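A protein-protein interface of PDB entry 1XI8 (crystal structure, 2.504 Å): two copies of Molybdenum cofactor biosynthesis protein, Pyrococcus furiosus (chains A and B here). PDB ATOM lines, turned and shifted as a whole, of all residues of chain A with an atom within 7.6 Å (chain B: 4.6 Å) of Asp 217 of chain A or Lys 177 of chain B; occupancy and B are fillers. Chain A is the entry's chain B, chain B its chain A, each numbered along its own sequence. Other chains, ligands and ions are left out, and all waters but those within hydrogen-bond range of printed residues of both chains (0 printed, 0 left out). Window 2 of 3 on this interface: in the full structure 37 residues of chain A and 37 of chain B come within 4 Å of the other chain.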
ATOM      1  N   ILE A 194       6.640  16.798  27.535  1.00  0.00           N
ATOM      2  CA  ILE A 194       5.448  15.968  27.536  1.00  0.00           C
ATOM      3  C   ILE A 194       5.844  14.530  27.767  1.00  0.00           C
ATOM      4  O   ILE A 194       6.552  13.941  26.966  1.00  0.00           O
ATOM      5  CB  ILE A 194       4.632  16.104  26.237  1.00  0.00           C
ATOM      6  CG1 ILE A 194       4.195  17.552  26.040  1.00  0.00           C
ATOM      7  CG2 ILE A 194       3.402  15.220  26.294  1.00  0.00           C
ATOM      8  CD1 ILE A 194       3.671  17.841  24.680  1.00  0.00           C
ATOM      9  N   ILE A 196       4.426  10.562  28.763  1.00  0.00           N
ATOM     10  CA  ILE A 196       3.215   9.726  28.712  1.00  0.00           C
ATOM     11  C   ILE A 196       3.362   8.283  29.232  1.00  0.00           C
ATOM     12  O   ILE A 196       4.105   7.468  28.672  1.00  0.00           O
ATOM     13  CB  ILE A 196       2.594   9.767  27.316  1.00  0.00           C
ATOM     14  CG1 ILE A 196       1.870  11.102  27.167  1.00  0.00           C
ATOM     15  CG2 ILE A 196       1.612   8.625  27.130  1.00  0.00           C
ATOM     16  CD1 ILE A 196       1.370  11.353  25.848  1.00  0.00           C
ATOM     17  N   THR A 197       2.615   7.993  30.301  1.00  0.00           N
ATOM     18  CA  THR A 197       2.741   6.760  31.084  1.00  0.00           C
ATOM     19  C   THR A 197       1.769   5.640  30.708  1.00  0.00           C
ATOM     20  O   THR A 197       0.560   5.859  30.677  1.00  0.00           O
ATOM     21  CB  THR A 197       2.494   7.076  32.573  1.00  0.00           C
ATOM     22  OG1 THR A 197       3.453   8.049  33.031  1.00  0.00           O
ATOM     23  CG2 THR A 197       2.577   5.794  33.421  1.00  0.00           C
ATOM     24  N   ASP A 217      -1.786   5.491  22.156  1.00  0.00           N
ATOM     25  CA  ASP A 217      -1.169   6.740  22.650  1.00  0.00           C
ATOM     26  C   ASP A 217      -1.503   7.933  21.771  1.00  0.00           C
ATOM     27  O   ASP A 217      -0.785   8.218  20.813  1.00  0.00           O
ATOM     28  CB  ASP A 217       0.355   6.630  22.756  1.00  0.00           C
ATOM     29  CG  ASP A 217       1.037   8.005  22.942  1.00  0.00           C
ATOM     30  OD1 ASP A 217       2.240   8.151  22.606  1.00  0.00           O
ATOM     31  OD2 ASP A 217       0.364   8.954  23.422  1.00  0.00           O
ATOM     32  N   THR A 218      -2.576   8.640  22.111  1.00  0.00           N
ATOM     33  CA  THR A 218      -3.012   9.799  21.331  1.00  0.00           C
ATOM     34  C   THR A 218      -2.695  11.163  22.007  1.00  0.00           C
ATOM     35  O   THR A 218      -2.569  12.196  21.341  1.00  0.00           O
ATOM     36  CB  THR A 218      -4.512   9.674  20.951  1.00  0.00           C
ATOM     37  OG1 THR A 218      -5.313   9.636  22.131  1.00  0.00           O
ATOM     38  CG2 THR A 218      -4.765   8.398  20.178  1.00  0.00           C
ATOM     39  N   ASN A 219      -2.549  11.156  23.325  1.00  0.00           N
ATOM     40  CA  ASN A 219      -2.289  12.393  24.068  1.00  0.00           C
ATOM     41  C   ASN A 219      -0.961  13.069  23.707  1.00  0.00           C
ATOM     42  O   ASN A 219      -0.830  14.289  23.748  1.00  0.00           O
ATOM     43  CB  ASN A 219      -2.368  12.132  25.575  1.00  0.00           C
ATOM     44  CG  ASN A 219      -3.755  11.697  26.021  1.00  0.00           C
ATOM     45  OD1 ASN A 219      -4.767  12.231  25.566  1.00  0.00           O
ATOM     46  ND2 ASN A 219      -3.807  10.732  26.917  1.00  0.00           N
ATOM     47  N   SER A 220       0.023  12.272  23.336  1.00  0.00           N
ATOM     48  CA  SER A 220       1.313  12.818  22.978  1.00  0.00           C
ATOM     49  C   SER A 220       1.219  13.826  21.837  1.00  0.00           C
ATOM     50  O   SER A 220       1.868  14.869  21.863  1.00  0.00           O
ATOM     51  CB  SER A 220       2.268  11.691  22.616  1.00  0.00           C
ATOM     52  OG  SER A 220       3.482  12.235  22.156  1.00  0.00           O
ATOM     53  N   ILE A 221       0.408  13.524  20.837  1.00  0.00           N
ATOM     54  CA  ILE A 221       0.268  14.442  19.730  1.00  0.00           C
ATOM     55  C   ILE A 221      -0.808  15.503  19.995  1.00  0.00           C
ATOM     56  O   ILE A 221      -0.714  16.627  19.516  1.00  0.00           O
ATOM     57  CB  ILE A 221       0.031  13.709  18.380  1.00  0.00           C
ATOM     58  CG1 ILE A 221       0.133  14.715  17.237  1.00  0.00           C
ATOM     59  CG2 ILE A 221      -1.317  12.992  18.360  1.00  0.00           C
ATOM     60  CD1 ILE A 221       0.482  14.116  15.930  1.00  0.00           C
ATOM     61  N   MET A 222      -1.823  15.154  20.774  1.00  0.00           N
ATOM     62  CA  MET A 222      -2.857  16.126  21.081  1.00  0.00           C
ATOM     63  C   MET A 222      -2.292  17.256  21.942  1.00  0.00           C
ATOM     64  O   MET A 222      -2.591  18.430  21.697  1.00  0.00           O
ATOM     65  CB  MET A 222      -4.050  15.479  21.775  1.00  0.00           C
ATOM     66  CG  MET A 222      -5.276  16.354  21.767  1.00  0.00           C
ATOM     67  SD  MET A 222      -6.549  15.783  22.896  1.00  0.00           S
ATOM     68  CE  MET A 222      -6.476  14.019  22.609  1.00  0.00           C
ATOM     69  N   LEU A 236       8.936  16.471  23.251  1.00  0.00           N
ATOM     70  CA  LEU A 236       8.308  15.169  23.346  1.00  0.00           C
ATOM     71  C   LEU A 236       9.217  14.047  23.858  1.00  0.00           C
ATOM     72  O   LEU A 236      10.014  13.498  23.091  1.00  0.00           O
ATOM     73  CB  LEU A 236       7.767  14.803  21.969  1.00  0.00           C
ATOM     74  CG  LEU A 236       6.650  13.777  21.977  1.00  0.00           C
ATOM     75  CD1 LEU A 236       5.787  13.994  23.233  1.00  0.00           C
ATOM     76  CD2 LEU A 236       5.853  13.889  20.673  1.00  0.00           C
ATOM     77  N   GLY A 238       8.110  11.263  24.667  1.00  0.00           N
ATOM     78  CA  GLY A 238       7.458  10.014  24.279  1.00  0.00           C
ATOM     79  C   GLY A 238       6.996   9.281  25.513  1.00  0.00           C
ATOM     80  O   GLY A 238       6.837   9.901  26.568  1.00  0.00           O
ATOM     81  N   VAL A 239       6.792   7.967  25.395  1.00  0.00           N
ATOM     82  CA  VAL A 239       6.228   7.184  26.493  1.00  0.00           C
ATOM     83  C   VAL A 239       7.268   6.739  27.515  1.00  0.00           C
ATOM     84  O   VAL A 239       8.471   6.668  27.232  1.00  0.00           O
ATOM     85  CB  VAL A 239       5.467   5.921  26.004  1.00  0.00           C
ATOM     86  CG1 VAL A 239       4.528   6.267  24.850  1.00  0.00           C
ATOM     87  CG2 VAL A 239       6.441   4.834  25.602  1.00  0.00           C
ATOM     88  N   THR A 264       1.059  12.318  31.851  1.00  0.00           N
ATOM     89  CA  THR A 264      -0.242  11.679  31.858  1.00  0.00           C
ATOM     90  C   THR A 264      -0.176  10.418  32.701  1.00  0.00           C
ATOM     91  O   THR A 264       0.849   9.731  32.718  1.00  0.00           O
ATOM     92  CB  THR A 264      -0.700  11.362  30.428  1.00  0.00           C
ATOM     93  OG1 THR A 264       0.287  10.560  29.777  1.00  0.00           O
ATOM     94  CG2 THR A 264      -0.886  12.645  29.635  1.00  0.00           C
ATOM     95  N   ILE A 373     -12.703  10.373  21.803  1.00  0.00           N
ATOM     96  CA  ILE A 373     -12.208  11.560  21.105  1.00  0.00           C
ATOM     97  C   ILE A 373     -13.266  12.298  20.243  1.00  0.00           C
ATOM     98  O   ILE A 373     -13.154  13.509  20.024  1.00  0.00           O
ATOM     99  CB  ILE A 373     -10.919  11.216  20.281  1.00  0.00           C
ATOM    100  CG1 ILE A 373      -9.953  10.390  21.138  1.00  0.00           C
ATOM    101  CG2 ILE A 373     -10.244  12.472  19.773  1.00  0.00           C
ATOM    102  CD1 ILE A 373      -8.606  10.094  20.501  1.00  0.00           C
ATOM    103  N   LEU B  39       1.762  13.455  10.974  1.00  0.00           N
ATOM    104  CA  LEU B  39       0.807  14.053  11.879  1.00  0.00           C
ATOM    105  C   LEU B  39       1.398  15.243  12.604  1.00  0.00           C
ATOM    106  O   LEU B  39       0.708  16.232  12.844  1.00  0.00           O
ATOM    107  CB  LEU B  39       0.327  13.021  12.884  1.00  0.00           C
ATOM    108  CG  LEU B  39      -0.820  12.118  12.458  1.00  0.00           C
ATOM    109  CD1 LEU B  39      -1.365  11.398  13.668  1.00  0.00           C
ATOM    110  CD2 LEU B  39      -1.912  12.942  11.834  1.00  0.00           C
ATOM    111  N   LEU B 173      -6.050  15.465  15.045  1.00  0.00           N
ATOM    112  CA  LEU B 173      -4.820  14.692  14.884  1.00  0.00           C
ATOM    113  C   LEU B 173      -4.816  13.483  15.824  1.00  0.00           C
ATOM    114  O   LEU B 173      -4.343  12.399  15.468  1.00  0.00           O
ATOM    115  CB  LEU B 173      -3.585  15.560  15.141  1.00  0.00           C
ATOM    116  CG  LEU B 173      -3.424  16.858  14.349  1.00  0.00           C
ATOM    117  CD1 LEU B 173      -2.127  17.540  14.756  1.00  0.00           C
ATOM    118  CD2 LEU B 173      -3.460  16.639  12.847  1.00  0.00           C
ATOM    119  N   ALA B 174      -5.345  13.680  17.027  1.00  0.00           N
ATOM    120  CA  ALA B 174      -5.444  12.606  17.994  1.00  0.00           C
ATOM    121  C   ALA B 174      -6.345  11.485  17.478  1.00  0.00           C
ATOM    122  O   ALA B 174      -6.069  10.311  17.718  1.00  0.00           O
ATOM    123  CB  ALA B 174      -5.943  13.132  19.326  1.00  0.00           C
ATOM    124  N   LEU B 175      -7.413  11.832  16.769  1.00  0.00           N
ATOM    125  CA  LEU B 175      -8.285  10.801  16.231  1.00  0.00           C
ATOM    126  C   LEU B 175      -7.589  10.046  15.091  1.00  0.00           C
ATOM    127  O   LEU B 175      -7.705   8.820  14.984  1.00  0.00           O
ATOM    128  CB  LEU B 175      -9.635  11.366  15.793  1.00  0.00           C
ATOM    129  CG  LEU B 175     -10.674  10.340  15.323  1.00  0.00           C
ATOM    130  CD1 LEU B 175     -10.826   9.191  16.321  1.00  0.00           C
ATOM    131  CD2 LEU B 175     -12.008  10.996  15.061  1.00  0.00           C
ATOM    132  N   LEU B 176      -6.849  10.774  14.258  1.00  0.00           N
ATOM    133  CA  LEU B 176      -6.085  10.153  13.190  1.00  0.00           C
ATOM    134  C   LEU B 176      -5.072   9.138  13.733  1.00  0.00           C
ATOM    135  O   LEU B 176      -4.932   8.034  13.185  1.00  0.00           O
ATOM    136  CB  LEU B 176      -5.403  11.221  12.331  1.00  0.00           C
ATOM    137  CG  LEU B 176      -6.411  12.041  11.520  1.00  0.00           C
ATOM    138  CD1 LEU B 176      -5.795  13.245  10.857  1.00  0.00           C
ATOM    139  CD2 LEU B 176      -7.068  11.150  10.491  1.00  0.00           C
ATOM    140  N   LYS B 177      -4.370   9.495  14.807  1.00  0.00           N
ATOM    141  CA  LYS B 177      -3.416   8.564  15.418  1.00  0.00           C
ATOM    142  C   LYS B 177      -4.133   7.305  15.873  1.00  0.00           C
ATOM    143  O   LYS B 177      -3.640   6.207  15.691  1.00  0.00           O
ATOM    144  CB  LYS B 177      -2.699   9.199  16.606  1.00  0.00           C
ATOM    145  CG  LYS B 177      -1.538   8.376  17.154  1.00  0.00           C
ATOM    146  CD  LYS B 177      -0.306   8.523  16.267  1.00  0.00           C
ATOM    147  CE  LYS B 177       0.837   7.623  16.718  1.00  0.00           C
ATOM    148  NZ  LYS B 177       1.998   7.707  15.765  1.00  0.00           N
ATOM    149  N   ALA B 178      -5.312   7.474  16.463  1.00  0.00           N
ATOM    150  CA  ALA B 178      -6.094   6.348  16.956  1.00  0.00           C
ATOM    151  C   ALA B 178      -6.466   5.420  15.812  1.00  0.00           C
ATOM    152  O   ALA B 178      -6.518   4.197  15.992  1.00  0.00           O
ATOM    153  CB  ALA B 178      -7.344   6.843  17.653  1.00  0.00           C
ATOM    154  N   LEU B 179      -6.721   6.014  14.642  1.00  0.00           N
ATOM    155  CA  LEU B 179      -7.119   5.272  13.454  1.00  0.00           C
ATOM    156  C   LEU B 179      -5.939   4.713  12.667  1.00  0.00           C
ATOM    157  O   LEU B 179      -6.132   3.955  11.726  1.00  0.00           O
ATOM    158  CB  LEU B 179      -7.988   6.139  12.557  1.00  0.00           C
ATOM    159  CG  LEU B 179      -9.391   6.356  13.106  1.00  0.00           C
ATOM    160  CD1 LEU B 179     -10.108   7.310  12.203  1.00  0.00           C
ATOM    161  CD2 LEU B 179     -10.150   5.024  13.214  1.00  0.00           C
ATOM    162  N   GLY B 180      -4.727   5.090  13.066  1.00  0.00           N
ATOM    163  CA  GLY B 180      -3.500   4.538  12.497  1.00  0.00           C
ATOM    164  C   GLY B 180      -3.042   5.220  11.229  1.00  0.00           C
ATOM    165  O   GLY B 180      -2.370   4.618  10.404  1.00  0.00           O
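Of chain B, only Lys 177 comes within 4 Å of Asp 217 of chain A. Printed residues of chain A within 4 Å of Lys 177 of chain B: Asp 217. Printed residues of chain B within 4 Å of Ile 221 of chain A: Leu 39. Of the printed residues of chain A, Ala 174 of chain B touches Thr 218 (3.4 Å), Met 222 (3.4 Å) and Ile 373 (3.8 Å). Of the printed residues of chain A, Ala 178 of chain B touches Thr 218. Of the printed residues of chain B, Met 222 of chain A touches Ala 174. Of the printed residues of chain B, Ile 373 of chain A touches Ala 174 (3.8 Å). The nearest residue of chain A that does not touch Lys 177 of chain B is Thr 218 of chain A (4.2 Å). The nearest printed residue of chain A that does not touch Ala 174 of chain B is Ile 221 of chain A (4.2 Å).
Asp 217 of chain A touches Lys 177 of chain B (O to CG, 3.7 Å). Thr 218 of chain A touches Ala 174 of chain B. CG2 of Thr 218 of chain A touches N of Ala 178 of chain B, at 3.9 Å. Ile 221 of chain A touches Leu 39 of chain B. Met 222 of chain A touches Ala 174 of chain B. CD1 of Ile 373 of chain A touches O of Ala 174 of chain B, 3.8 Å away.
No position is printed for both chains. Of the 6 pairs that touch across the chains among the printed residues, none has its exchanged pair printed and touching as well.
The side-chain carboxylate (OD2) of Asp 217 of chain A sits at hydrogen-bond distance from the backbone NH (N) of Ser 220 of chain A, 3.3 Å away.
Hydrophobic or aromatic side chains of chain B that line the printed part of chain A: Leu 39, Ala 174 and Ala 178. Printed residues of chain A that touch a printed residue of chain B: Asp 217, Thr 218, Ile 221, Met 222 and Ile 373. Among the printed residues, 6 pairs touch across the chains. Among the printed residues, no Asp or Glu carboxylate lies within 4 Å of a Lys or Arg side-chain nitrogen of the other chain.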
